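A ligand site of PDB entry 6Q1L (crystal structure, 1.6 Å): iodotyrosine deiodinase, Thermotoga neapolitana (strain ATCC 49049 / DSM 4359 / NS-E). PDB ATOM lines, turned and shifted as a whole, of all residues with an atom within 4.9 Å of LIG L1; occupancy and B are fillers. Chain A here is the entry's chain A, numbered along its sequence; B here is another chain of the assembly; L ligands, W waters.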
ATOM      1  N   ARG A  11     -13.832 -35.066  12.533  1.00  0.00           N
ATOM      2  CA  ARG A  11     -14.174 -33.741  12.990  1.00  0.00           C
ATOM      3  C   ARG A  11     -14.585 -32.859  11.830  1.00  0.00           C
ATOM      4  O   ARG A  11     -13.912 -32.850  10.789  1.00  0.00           O
ATOM      5  CB  ARG A  11     -13.015 -33.061  13.711  1.00  0.00           C
ATOM      6  CG  ARG A  11     -13.515 -31.619  13.769  1.00  0.00           C
ATOM      7  CD  ARG A  11     -12.585 -30.529  13.837  1.00  0.00           C
ATOM      8  NE  ARG A  11     -13.377 -29.375  14.273  1.00  0.00           N
ATOM      9  CZ  ARG A  11     -13.857 -28.436  13.475  1.00  0.00           C
ATOM     10  NH1 ARG A  11     -13.663 -28.472  12.161  1.00  0.00           N
ATOM     11  NH2 ARG A  11     -14.558 -27.430  13.976  1.00  0.00           N
ATOM     12  N   LYS A  12     -15.679 -32.131  12.003  1.00  0.00           N
ATOM     13  CA  LYS A  12     -16.249 -31.271  10.992  1.00  0.00           C
ATOM     14  C   LYS A  12     -16.835 -30.053  11.682  1.00  0.00           C
ATOM     15  O   LYS A  12     -17.049 -30.045  12.895  1.00  0.00           O
ATOM     16  CB  LYS A  12     -17.315 -31.994  10.189  1.00  0.00           C
ATOM     17  CG  LYS A  12     -18.573 -32.371  10.981  1.00  0.00           C
ATOM     18  CD  LYS A  12     -19.511 -33.166  10.107  1.00  0.00           C
ATOM     19  CE  LYS A  12     -20.739 -33.670  10.839  1.00  0.00           C
ATOM     20  NZ  LYS A  12     -20.408 -34.715  11.837  1.00  0.00           N
ATOM     21  N   THR A  13     -17.168 -29.037  10.884  1.00  0.00           N
ATOM     22  CA  THR A  13     -17.796 -27.844  11.426  1.00  0.00           C
ATOM     23  C   THR A  13     -19.099 -28.227  12.115  1.00  0.00           C
ATOM     24  O   THR A  13     -19.841 -29.089  11.652  1.00  0.00           O
ATOM     25  CB  THR A  13     -18.101 -26.839  10.327  1.00  0.00           C
ATOM     26  OG1 THR A  13     -17.038 -26.800   9.389  1.00  0.00           O
ATOM     27  CG2 THR A  13     -18.277 -25.443  10.917  1.00  0.00           C
ATOM     28  N   ARG A  15     -22.279 -25.917  13.247  1.00  0.00           N
ATOM     29  CA  ARG A  15     -22.943 -24.639  13.337  1.00  0.00           C
ATOM     30  C   ARG A  15     -24.328 -24.772  13.967  1.00  0.00           C
ATOM     31  O   ARG A  15     -25.031 -23.765  14.098  1.00  0.00           O
ATOM     32  CB  ARG A  15     -23.068 -23.983  11.964  1.00  0.00           C
ATOM     33  CG  ARG A  15     -21.714 -23.721  11.321  1.00  0.00           C
ATOM     34  CD  ARG A  15     -21.848 -23.081   9.980  1.00  0.00           C
ATOM     35  NE  ARG A  15     -20.561 -22.838   9.323  1.00  0.00           N
ATOM     36  CZ  ARG A  15     -19.925 -23.667   8.520  1.00  0.00           C
ATOM     37  NH1 ARG A  15     -20.425 -24.885   8.212  1.00  0.00           N
ATOM     38  NH2 ARG A  15     -18.767 -23.278   8.000  1.00  0.00           N
ATOM     39  N   GLU A  68     -21.532  -8.892   9.210  1.00  0.00           N
ATOM     40  CA  GLU A  68     -21.719  -9.901   8.172  1.00  0.00           C
ATOM     41  C   GLU A  68     -22.706  -9.416   7.122  1.00  0.00           C
ATOM     42  O   GLU A  68     -22.510  -9.619   5.920  1.00  0.00           O
ATOM     43  CB  GLU A  68     -22.230 -11.206   8.763  1.00  0.00           C
ATOM     44  CG  GLU A  68     -21.290 -11.939   9.674  1.00  0.00           C
ATOM     45  CD  GLU A  68     -20.105 -12.510   8.942  1.00  0.00           C
ATOM     46  OE1 GLU A  68     -19.924 -12.171   7.748  1.00  0.00           O
ATOM     47  OE2 GLU A  68     -19.353 -13.297   9.575  1.00  0.00           O
ATOM     48  N   TRP A  82     -18.430 -19.393  -3.234  1.00  0.00           N
ATOM     49  CA  TRP A  82     -18.505 -20.500  -2.310  1.00  0.00           C
ATOM     50  C   TRP A  82     -19.630 -20.317  -1.293  1.00  0.00           C
ATOM     51  O   TRP A  82     -20.400 -21.246  -1.032  1.00  0.00           O
ATOM     52  CB  TRP A  82     -17.141 -20.638  -1.609  1.00  0.00           C
ATOM     53  CG  TRP A  82     -16.991 -21.804  -0.759  1.00  0.00           C
ATOM     54  CD1 TRP A  82     -16.560 -23.037  -1.124  1.00  0.00           C
ATOM     55  CD2 TRP A  82     -17.201 -21.856   0.658  1.00  0.00           C
ATOM     56  NE1 TRP A  82     -16.508 -23.860  -0.037  1.00  0.00           N
ATOM     57  CE2 TRP A  82     -16.897 -23.159   1.078  1.00  0.00           C
ATOM     58  CE3 TRP A  82     -17.620 -20.933   1.605  1.00  0.00           C
ATOM     59  CZ2 TRP A  82     -16.994 -23.574   2.395  1.00  0.00           C
ATOM     60  CZ3 TRP A  82     -17.723 -21.339   2.935  1.00  0.00           C
ATOM     61  CH2 TRP A  82     -17.413 -22.650   3.306  1.00  0.00           C
ATOM     62  N   PHE A  88     -24.881 -19.956   2.590  1.00  0.00           N
ATOM     63  CA  PHE A  88     -24.581 -19.175   3.782  1.00  0.00           C
ATOM     64  C   PHE A  88     -25.323 -17.842   3.762  1.00  0.00           C
ATOM     65  O   PHE A  88     -25.605 -17.267   2.706  1.00  0.00           O
ATOM     66  CB  PHE A  88     -23.087 -18.884   3.883  1.00  0.00           C
ATOM     67  CG  PHE A  88     -22.229 -20.037   4.385  1.00  0.00           C
ATOM     68  CD1 PHE A  88     -22.060 -21.179   3.643  1.00  0.00           C
ATOM     69  CD2 PHE A  88     -21.516 -19.914   5.548  1.00  0.00           C
ATOM     70  CE1 PHE A  88     -21.238 -22.204   4.088  1.00  0.00           C
ATOM     71  CE2 PHE A  88     -20.690 -20.948   5.993  1.00  0.00           C
ATOM     72  CZ  PHE A  88     -20.576 -22.083   5.270  1.00  0.00           C
ATOM     73  N   TRP A 118      -2.861 -20.051  16.224  1.00  0.00           N
ATOM     74  CA  TRP A 118      -3.652 -20.865  15.301  1.00  0.00           C
ATOM     75  C   TRP A 118      -3.220 -22.329  15.336  1.00  0.00           C
ATOM     76  O   TRP A 118      -4.049 -23.230  15.221  1.00  0.00           O
ATOM     77  CB  TRP A 118      -3.588 -20.243  13.893  1.00  0.00           C
ATOM     78  CG  TRP A 118      -4.585 -19.167  13.828  1.00  0.00           C
ATOM     79  CD1 TRP A 118      -4.369 -17.842  13.959  1.00  0.00           C
ATOM     80  CD2 TRP A 118      -5.995 -19.319  13.678  1.00  0.00           C
ATOM     81  NE1 TRP A 118      -5.546 -17.155  13.918  1.00  0.00           N
ATOM     82  CE2 TRP A 118      -6.565 -18.053  13.761  1.00  0.00           C
ATOM     83  CE3 TRP A 118      -6.811 -20.421  13.485  1.00  0.00           C
ATOM     84  CZ2 TRP A 118      -7.921 -17.852  13.589  1.00  0.00           C
ATOM     85  CZ3 TRP A 118      -8.150 -20.212  13.359  1.00  0.00           C
ATOM     86  CH2 TRP A 118      -8.688 -18.943  13.435  1.00  0.00           C
ATOM     87  N   VAL A 136     -17.002 -24.170  15.493  1.00  0.00           N
ATOM     88  CA  VAL A 136     -16.720 -23.573  14.187  1.00  0.00           C
ATOM     89  C   VAL A 136     -15.765 -22.411  14.449  1.00  0.00           C
ATOM     90  O   VAL A 136     -16.008 -21.593  15.351  1.00  0.00           O
ATOM     91  CB  VAL A 136     -18.009 -23.104  13.479  1.00  0.00           C
ATOM     92  CG1 VAL A 136     -18.858 -22.233  14.400  1.00  0.00           C
ATOM     93  CG2 VAL A 136     -17.629 -22.429  12.178  1.00  0.00           C
ATOM     94  N   PRO A 137     -14.665 -22.283  13.694  1.00  0.00           N
ATOM     95  CA  PRO A 137     -13.816 -21.099  13.823  1.00  0.00           C
ATOM     96  C   PRO A 137     -14.478 -19.918  13.172  1.00  0.00           C
ATOM     97  O   PRO A 137     -14.380 -19.737  11.959  1.00  0.00           O
ATOM     98  CB  PRO A 137     -12.536 -21.495  13.099  1.00  0.00           C
ATOM     99  CG  PRO A 137     -12.617 -22.988  12.951  1.00  0.00           C
ATOM    100  CD  PRO A 137     -14.088 -23.232  12.729  1.00  0.00           C
ATOM    101  N   TYR A 138     -15.204 -19.151  13.937  1.00  0.00           N
ATOM    102  CA  TYR A 138     -15.990 -18.062  13.383  1.00  0.00           C
ATOM    103  C   TYR A 138     -15.151 -16.790  13.354  1.00  0.00           C
ATOM    104  O   TYR A 138     -14.585 -16.388  14.369  1.00  0.00           O
ATOM    105  CB  TYR A 138     -17.266 -17.865  14.201  1.00  0.00           C
ATOM    106  CG  TYR A 138     -18.003 -16.690  13.680  1.00  0.00           C
ATOM    107  CD1 TYR A 138     -18.441 -16.650  12.347  1.00  0.00           C
ATOM    108  CD2 TYR A 138     -18.254 -15.609  14.487  1.00  0.00           C
ATOM    109  CE1 TYR A 138     -19.075 -15.560  11.856  1.00  0.00           C
ATOM    110  CE2 TYR A 138     -18.894 -14.489  13.992  1.00  0.00           C
ATOM    111  CZ  TYR A 138     -19.316 -14.476  12.680  1.00  0.00           C
ATOM    112  OH  TYR A 138     -19.957 -13.367  12.176  1.00  0.00           O
ATOM    113  N   THR A 139     -15.044 -16.188  12.176  1.00  0.00           N
ATOM    114  CA  THR A 139     -14.214 -15.013  11.961  1.00  0.00           C
ATOM    115  C   THR A 139     -15.074 -13.934  11.334  1.00  0.00           C
ATOM    116  O   THR A 139     -15.192 -13.861  10.099  1.00  0.00           O
ATOM    117  CB  THR A 139     -12.987 -15.330  11.106  1.00  0.00           C
ATOM    118  OG1 THR A 139     -13.408 -15.912   9.879  1.00  0.00           O
ATOM    119  CG2 THR A 139     -12.038 -16.284  11.827  1.00  0.00           C
ATOM    120  N   PRO A 140     -15.690 -13.074  12.130  1.00  0.00           N
ATOM    121  CA  PRO A 140     -16.549 -12.008  11.589  1.00  0.00           C
ATOM    122  C   PRO A 140     -15.704 -10.944  10.915  1.00  0.00           C
ATOM    123  O   PRO A 140     -14.496 -10.842  11.175  1.00  0.00           O
ATOM    124  CB  PRO A 140     -17.243 -11.439  12.836  1.00  0.00           C
ATOM    125  CG  PRO A 140     -16.164 -11.598  13.918  1.00  0.00           C
ATOM    126  CD  PRO A 140     -15.518 -12.964  13.598  1.00  0.00           C
ATOM    127  N   PRO A 172     -23.020 -32.443   6.942  1.00  0.00           N
ATOM    128  CA  PRO A 172     -21.875 -33.321   6.667  1.00  0.00           C
ATOM    129  C   PRO A 172     -20.595 -32.544   6.409  1.00  0.00           C
ATOM    130  O   PRO A 172     -20.609 -31.393   5.958  1.00  0.00           O
ATOM    131  CB  PRO A 172     -22.294 -34.087   5.412  1.00  0.00           C
ATOM    132  CG  PRO A 172     -23.800 -33.957   5.371  1.00  0.00           C
ATOM    133  CD  PRO A 172     -24.124 -32.629   5.984  1.00  0.00           C
ATOM    134  N   LYS A 173     -19.477 -33.209   6.695  1.00  0.00           N
ATOM    135  CA  LYS A 173     -18.178 -32.653   6.372  1.00  0.00           C
ATOM    136  C   LYS A 173     -18.056 -32.430   4.872  1.00  0.00           C
ATOM    137  O   LYS A 173     -18.554 -33.225   4.077  1.00  0.00           O
ATOM    138  CB  LYS A 173     -17.080 -33.586   6.855  1.00  0.00           C
ATOM    139  CG  LYS A 173     -15.689 -32.921   6.843  1.00  0.00           C
ATOM    140  CD  LYS A 173     -14.708 -33.805   7.564  1.00  0.00           C
ATOM    141  CE  LYS A 173     -13.393 -33.056   7.649  1.00  0.00           C
ATOM    142  NZ  LYS A 173     -12.336 -33.699   8.433  1.00  0.00           N
ATOM    143  N   TYR A 174     -17.433 -31.311   4.497  1.00  0.00           N
ATOM    144  CA  TYR A 174     -17.215 -31.014   3.088  1.00  0.00           C
ATOM    145  C   TYR A 174     -16.070 -31.885   2.596  1.00  0.00           C
ATOM    146  O   TYR A 174     -15.310 -32.432   3.381  1.00  0.00           O
ATOM    147  CB  TYR A 174     -16.884 -29.549   2.865  1.00  0.00           C
ATOM    148  CG  TYR A 174     -17.982 -28.565   3.241  1.00  0.00           C
ATOM    149  CD1 TYR A 174     -19.313 -28.940   3.253  1.00  0.00           C
ATOM    150  CD2 TYR A 174     -17.683 -27.253   3.552  1.00  0.00           C
ATOM    151  CE1 TYR A 174     -20.306 -28.072   3.570  1.00  0.00           C
ATOM    152  CE2 TYR A 174     -18.679 -26.343   3.909  1.00  0.00           C
ATOM    153  CZ  TYR A 174     -19.990 -26.763   3.920  1.00  0.00           C
ATOM    154  OH  TYR A 174     -20.985 -25.885   4.259  1.00  0.00           O
ATOM    155  N   ARG A 176     -12.555 -33.299   0.853  1.00  0.00           N
ATOM    156  CA  ARG A 176     -11.165 -32.900   0.919  1.00  0.00           C
ATOM    157  C   ARG A 176     -10.503 -33.384  -0.354  1.00  0.00           C
ATOM    158  O   ARG A 176     -10.574 -34.560  -0.681  1.00  0.00           O
ATOM    159  CB  ARG A 176     -10.439 -33.498   2.118  1.00  0.00           C
ATOM    160  CG  ARG A 176     -10.868 -32.932   3.457  1.00  0.00           C
ATOM    161  CD  ARG A 176     -10.564 -31.480   3.611  1.00  0.00           C
ATOM    162  NE  ARG A 176     -10.755 -31.016   4.974  1.00  0.00           N
ATOM    163  CZ  ARG A 176     -11.939 -30.669   5.486  1.00  0.00           C
ATOM    164  NH1 ARG A 176     -13.043 -30.774   4.746  1.00  0.00           N
ATOM    165  NH2 ARG A 176     -12.018 -30.215   6.723  1.00  0.00           N
ATOM    166  N   GLU B  36      -7.105 -33.071   6.755  1.00  0.00           N
ATOM    167  CA  GLU B  36      -8.460 -33.186   7.255  1.00  0.00           C
ATOM    168  C   GLU B  36      -8.870 -31.991   8.083  1.00  0.00           C
ATOM    169  O   GLU B  36     -10.032 -31.906   8.489  1.00  0.00           O
ATOM    170  CB  GLU B  36      -8.599 -34.473   8.082  1.00  0.00           C
ATOM    171  CG  GLU B  36      -8.475 -35.710   7.270  1.00  0.00           C
ATOM    172  CD  GLU B  36      -9.635 -35.867   6.326  1.00  0.00           C
ATOM    173  OE1 GLU B  36     -10.744 -35.426   6.674  1.00  0.00           O
ATOM    174  OE2 GLU B  36      -9.456 -36.410   5.205  1.00  0.00           O
ATOM    175  N   PRO B  38      -9.940 -28.238   9.211  1.00  0.00           N
ATOM    176  CA  PRO B  38     -10.715 -27.165   8.607  1.00  0.00           C
ATOM    177  C   PRO B  38      -9.830 -26.085   8.000  1.00  0.00           C
ATOM    178  O   PRO B  38      -8.613 -25.990   8.268  1.00  0.00           O
ATOM    179  CB  PRO B  38     -11.523 -26.613   9.795  1.00  0.00           C
ATOM    180  CG  PRO B  38     -10.578 -26.814  10.992  1.00  0.00           C
ATOM    181  CD  PRO B  38      -9.917 -28.175  10.698  1.00  0.00           C
ATOM    182  N   SER B  39     -10.451 -25.253   7.158  1.00  0.00           N
ATOM    183  CA  SER B  39      -9.766 -24.121   6.564  1.00  0.00           C
ATOM    184  C   SER B  39     -10.809 -23.119   6.091  1.00  0.00           C
ATOM    185  O   SER B  39     -11.965 -23.472   5.849  1.00  0.00           O
ATOM    186  CB  SER B  39      -8.848 -24.569   5.414  1.00  0.00           C
ATOM    187  OG  SER B  39      -9.610 -25.169   4.362  1.00  0.00           O
ATOM    188  N   GLY B  40     -10.364 -21.889   5.928  1.00  0.00           N
ATOM    189  CA  GLY B  40     -11.248 -20.848   5.445  1.00  0.00           C
ATOM    190  C   GLY B  40     -11.787 -21.260   4.093  1.00  0.00           C
ATOM    191  O   GLY B  40     -11.022 -21.654   3.225  1.00  0.00           O
ATOM    192  N   MET B  41     -13.105 -21.238   3.928  1.00  0.00           N
ATOM    193  CA  MET B  41     -13.732 -21.560   2.643  1.00  0.00           C
ATOM    194  C   MET B  41     -13.432 -22.993   2.202  1.00  0.00           C
ATOM    195  O   MET B  41     -13.635 -23.345   1.027  1.00  0.00           O
ATOM    196  CB  MET B  41     -13.235 -20.566   1.588  1.00  0.00           C
ATOM    197  CG  MET B  41     -14.034 -20.428   0.330  1.00  0.00           C
ATOM    198  SD  MET B  41     -13.117 -19.286  -0.740  1.00  0.00           S
ATOM    199  CE  MET B  41     -13.466 -20.044  -2.314  1.00  0.00           C
ATOM    200  N   ASN B  42     -13.006 -23.850   3.144  1.00  0.00           N
ATOM    201  CA  ASN B  42     -12.541 -25.200   2.822  1.00  0.00           C
ATOM    202  C   ASN B  42     -11.547 -25.164   1.676  1.00  0.00           C
ATOM    203  O   ASN B  42     -11.517 -26.057   0.814  1.00  0.00           O
ATOM    204  CB  ASN B  42     -13.696 -26.154   2.476  1.00  0.00           C
ATOM    205  CG  ASN B  42     -13.275 -27.613   2.517  1.00  0.00           C
ATOM    206  OD1 ASN B  42     -12.413 -28.003   3.309  1.00  0.00           O
ATOM    207  ND2 ASN B  42     -13.876 -28.420   1.680  1.00  0.00           N
ATOM    208  N   TYR B 112      -8.129 -16.391   4.910  1.00  0.00           N
ATOM    209  CA  TYR B 112      -7.606 -16.940   6.172  1.00  0.00           C
ATOM    210  C   TYR B 112      -6.633 -18.082   5.886  1.00  0.00           C
ATOM    211  O   TYR B 112      -6.523 -19.056   6.641  1.00  0.00           O
ATOM    212  CB  TYR B 112      -8.742 -17.375   7.095  1.00  0.00           C
ATOM    213  CG  TYR B 112      -9.274 -16.213   7.897  1.00  0.00           C
ATOM    214  CD1 TYR B 112     -10.250 -15.377   7.388  1.00  0.00           C
ATOM    215  CD2 TYR B 112      -8.752 -15.927   9.159  1.00  0.00           C
ATOM    216  CE1 TYR B 112     -10.708 -14.289   8.115  1.00  0.00           C
ATOM    217  CE2 TYR B 112      -9.209 -14.861   9.891  1.00  0.00           C
ATOM    218  CZ  TYR B 112     -10.180 -14.044   9.360  1.00  0.00           C
ATOM    219  OH  TYR B 112     -10.636 -12.966  10.101  1.00  0.00           O
ATOM    220  N   GLU B 115      -3.800 -18.454   8.729  1.00  0.00           N
ATOM    221  CA  GLU B 115      -4.439 -19.033   9.900  1.00  0.00           C
ATOM    222  C   GLU B 115      -4.735 -20.503   9.708  1.00  0.00           C
ATOM    223  O   GLU B 115      -4.494 -21.343  10.568  1.00  0.00           O
ATOM    224  CB  GLU B 115      -5.743 -18.294  10.174  1.00  0.00           C
ATOM    225  CG  GLU B 115      -5.514 -16.874  10.608  1.00  0.00           C
ATOM    226  CD  GLU B 115      -5.391 -15.870   9.442  1.00  0.00           C
ATOM    227  OE1 GLU B 115      -5.363 -16.281   8.236  1.00  0.00           O
ATOM    228  OE2 GLU B 115      -5.358 -14.644   9.732  1.00  0.00           O
ATOM    229  N   SER B 116      -5.330 -20.836   8.550  1.00  0.00           N
ATOM    230  CA  SER B 116      -5.711 -22.211   8.304  1.00  0.00           C
ATOM    231  C   SER B 116      -4.500 -23.119   8.211  1.00  0.00           C
ATOM    232  O   SER B 116      -4.553 -24.266   8.642  1.00  0.00           O
ATOM    233  CB  SER B 116      -6.499 -22.319   6.992  1.00  0.00           C
ATOM    234  OG  SER B 116      -7.698 -21.557   7.005  1.00  0.00           O
ATOM    235  N   LEU B 119      -3.178 -23.737  11.728  1.00  0.00           N
ATOM    236  CA  LEU B 119      -4.072 -24.690  12.369  1.00  0.00           C
ATOM    237  C   LEU B 119      -3.723 -26.112  11.931  1.00  0.00           C
ATOM    238  O   LEU B 119      -3.611 -27.031  12.744  1.00  0.00           O
ATOM    239  CB  LEU B 119      -5.509 -24.321  12.013  1.00  0.00           C
ATOM    240  CG  LEU B 119      -6.636 -25.032  12.748  1.00  0.00           C
ATOM    241  CD1 LEU B 119      -7.898 -24.197  12.686  1.00  0.00           C
ATOM    242  CD2 LEU B 119      -6.877 -26.444  12.211  1.00  0.00           C
HETATM  243  N1  LIG L   1     -17.083 -20.964   9.081  1.00  0.00           N
HETATM  244  C1  LIG L   1     -18.088 -20.027   9.114  1.00  0.00           C
HETATM  245  O1  LIG L   1     -19.255 -20.367   9.030  1.00  0.00           O
HETATM  246  N2  LIG L   1     -17.787 -18.708   9.267  1.00  0.00           N
HETATM  247  C2  LIG L   1     -16.521 -18.245   9.368  1.00  0.00           C
HETATM  248  O2  LIG L   1     -16.334 -17.032   9.496  1.00  0.00           O
HETATM  249  C3  LIG L   1     -15.510 -19.191   9.321  1.00  0.00           C
HETATM  250  N3  LIG L   1     -14.203 -18.775   9.410  1.00  0.00           N
HETATM  251  C4  LIG L   1     -13.202 -19.705   9.414  1.00  0.00           C
HETATM  252  C5  LIG L   1     -11.883 -19.253   9.545  1.00  0.00           C
HETATM  253  C6  LIG L   1     -10.840 -20.174   9.557  1.00  0.00           C
HETATM  254  C7  LIG L   1      -9.407 -19.693   9.720  1.00  0.00           C
HETATM  255  C8  LIG L   1     -11.119 -21.549   9.416  1.00  0.00           C
HETATM  256  C9  LIG L   1     -10.004 -22.582   9.436  1.00  0.00           C
HETATM  257  C10 LIG L   1     -12.442 -21.993   9.285  1.00  0.00           C
HETATM  258  C11 LIG L   1     -13.474 -21.055   9.262  1.00  0.00           C
HETATM  259  N4  LIG L   1     -14.798 -21.476   9.126  1.00  0.00           N
HETATM  260  C12 LIG L   1     -15.800 -20.527   9.190  1.00  0.00           C
HETATM  261  C13 LIG L   1     -15.163 -22.901   8.942  1.00  0.00           C
HETATM  262  C14 LIG L   1     -14.859 -23.322   7.489  1.00  0.00           C
HETATM  263  O3  LIG L   1     -15.908 -22.882   6.654  1.00  0.00           O
HETATM  264  C15 LIG L   1     -14.758 -24.847   7.500  1.00  0.00           C
HETATM  265  O4  LIG L   1     -13.634 -25.229   8.275  1.00  0.00           O
HETATM  266  C16 LIG L   1     -14.674 -25.503   6.118  1.00  0.00           C
HETATM  267  O5  LIG L   1     -15.899 -25.237   5.456  1.00  0.00           O
HETATM  268  C17 LIG L   1     -14.443 -26.994   6.222  1.00  0.00           C
HETATM  269  O6  LIG L   1     -15.484 -27.633   6.959  1.00  0.00           O
HETATM  270  P1  LIG L   1     -15.408 -29.189   7.209  1.00  0.00           P
HETATM  271  O7  LIG L   1     -16.763 -29.398   7.923  1.00  0.00           O
HETATM  272  O8  LIG L   1     -14.278 -29.548   8.081  1.00  0.00           O
HETATM  273  O9  LIG L   1     -15.406 -29.860   5.831  1.00  0.00           O
HETATM  274  N1  LG2 L   2     -17.739 -15.070   8.184  1.00  0.00           N
HETATM  275  C1  LG2 L   2     -18.740 -15.251   7.151  1.00  0.00           C
HETATM  276  C2  LG2 L   2     -18.169 -15.808   5.832  1.00  0.00           C
HETATM  277  C3  LG2 L   2     -17.338 -17.037   5.915  1.00  0.00           C
HETATM  278  C4  LG2 L   2     -15.961 -16.945   5.778  1.00  0.00           C
HETATM  279  C5  LG2 L   2     -15.170 -18.092   5.805  1.00  0.00           C
HETATM  280  I1  LG2 L   2     -13.189 -17.814   5.675  1.00  0.00           I
HETATM  281  C6  LG2 L   2     -15.741 -19.334   5.952  1.00  0.00           C
HETATM  282  O1  LG2 L   2     -15.035 -20.487   5.985  1.00  0.00           O
HETATM  283  C7  LG2 L   2     -17.127 -19.452   6.078  1.00  0.00           C
HETATM  284  C8  LG2 L   2     -17.918 -18.305   6.050  1.00  0.00           C
HETATM  285  C9  LG2 L   2     -19.835 -16.181   7.621  1.00  0.00           C
HETATM  286  O2  LG2 L   2     -20.894 -16.435   7.009  1.00  0.00           O
HETATM  287  O3  LG2 L   2     -19.631 -16.828   8.777  1.00  0.00           O
HETATM  288  O   HOH W   1     -21.815 -19.435   9.120  1.00  0.00           O
HETATM  289  O   HOH W   2     -19.106 -28.962   6.976  1.00  0.00           O
HETATM  290  O   HOH W   3     -18.108 -26.192   7.059  1.00  0.00           O
HETATM  291  O   HOH W   4     -12.777 -30.282  10.157  1.00  0.00           O
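NH1 of Arg 176 is in hydrogen-bond range of O of Tyr 174 (3.1 Å).
The side-chain amide oxygen (OD1) of Asn 42 of chain B lies within hydrogen-bond range of the guanidinium group (NH1) of Arg 176 (3.2 Å).
The guanidinium group of Arg 176 sits at hydrogen-bond distance from the backbone carbonyl oxygen of Glu 36 of chain B (3.1 Å).
NZ of Lys 173 is in hydrogen-bond range of O of Arg 11.
The side-chain amino group of Lys 173 lies within salt-bridge range of the side-chain carboxylate of Glu 36 of chain B (2.9 Å).
The backbone carbonyl oxygen (O) of Tyr 112 of chain B lies within hydrogen-bond range of the side-chain hydroxyl (OG) of Ser 116 of chain B (2.8 Å).
The side-chain hydroxyl (OG) of Ser 116 of chain B lies within hydrogen-bond range of the backbone NH (N) of Gly 40 of chain B (2.9 Å).
The side-chain hydroxyl of Tyr 138 lies within hydrogen-bond range of the side-chain carboxylate of Glu 68 (2.7 Å).
The guanidinium group of Arg 176 is in salt-bridge range of an oxygen (O8) of LIG L1, at 2.7 Å.
O of Pro 137 sits close to N3 of LIG L1.
NE of Arg 15 lies within hydrogen-bond range of O1 of LIG L1, at 2.8 Å.
N of Tyr 174 lies within hydrogen-bond range of O9 of LIG L1.
The backbone NH (N) of Thr 13 is in hydrogen-bond range of an oxygen (O7) of LIG L1 (3.0 Å).
The side-chain hydroxyl (OG1) of Thr 13 sits at hydrogen-bond distance from an oxygen (O7) of LIG L1 (3.0 Å).
The backbone NH (N) of Thr 139 lies within hydrogen-bond range of an oxygen (O2) of LIG L1.
OG1 of Thr 139 sits at hydrogen-bond distance from N3 of LIG L1 (3.0 Å).
An oxygen (O4) of LIG L1 lies within hydrogen-bond range of the backbone NH of Ser 39 of chain B (3.4 Å).
An oxygen (O4) of LIG L1 sits close to the backbone carbonyl oxygen (O) of Ser 39 of chain B, 3.4 Å away.
The backbone carbonyl oxygen (O) of Thr 139 lies within hydrogen-bond range of a nitrogen (N1) of LG2 L2, at 3.4 Å.
N of Met 41 of chain B sits at hydrogen-bond distance from O1 of LG2 L2, 2.9 Å away.
A nitrogen (N1) of LG2 L2 is in salt-bridge range of the side-chain carboxylate (OE2) of Glu 68, 2.8 Å away.
O1 of LG2 L2 sits at hydrogen-bond distance from O3 of LIG L1, 2.6 Å away.
Lys 12 touches LIG L1.
CZ2 of Trp 82 touches O5 of LIG L1 (3.7 Å).
Phe 88 touches LIG L1.
Trp 118 touches LIG L1 (CH2 to C7, 3.9 Å).
Val 136 touches LIG L1 (CG2 to N1, 3.5 Å).
Tyr 138 touches LIG L1.
CG of Lys 173 touches O9 of LIG L1, at 3.2 Å.
Pro 38 of chain B touches LIG L1.
N of Gly 40 of chain B touches C8 of LIG L1, at 3.6 Å.
OD1 of Asn 42 of chain B touches C17 of LIG L1, 3.7 Å away.
Tyr 112 of chain B touches LIG L1 (CB to C7, 3.6 Å).
Glu 115 of chain B touches LIG L1 (CB to C7, 3.9 Å).
OG of Ser 116 of chain B touches C9 of LIG L1, at 3.5 Å.
Hydrophobic or aromatic side chains that line LIG L1: Trp 82, Phe 88, Trp 118, Val 136, Pro 137, Tyr 138, Tyr 174, Pro 38 of chain B and Tyr 112 of chain B.
Of the 27 residues printed, 20 come within 4 Å of LIG L1.
The nearest printed residue that does not touch LIG L1 is Leu 119 of chain B (4.2 Å).
Water W2 lies within hydrogen-bond range of O7 of LIG L1 (2.6 Å) and O of Pro 172 (3.0 Å).
Water W4 lies within hydrogen-bond range of O8 of LIG L1 and NH1 of Arg 11.
Water W1 bridges an oxygen (O1) of LIG L1 (2.7 Å) and an oxygen (O3) of LG2 L2 (3.4 Å).
Water W3 lies within hydrogen-bond range of OG1 of Thr 13 (2.6 Å), O5 of LIG L1 (2.9 Å) and NH1 of Arg 15 (2.9 Å).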
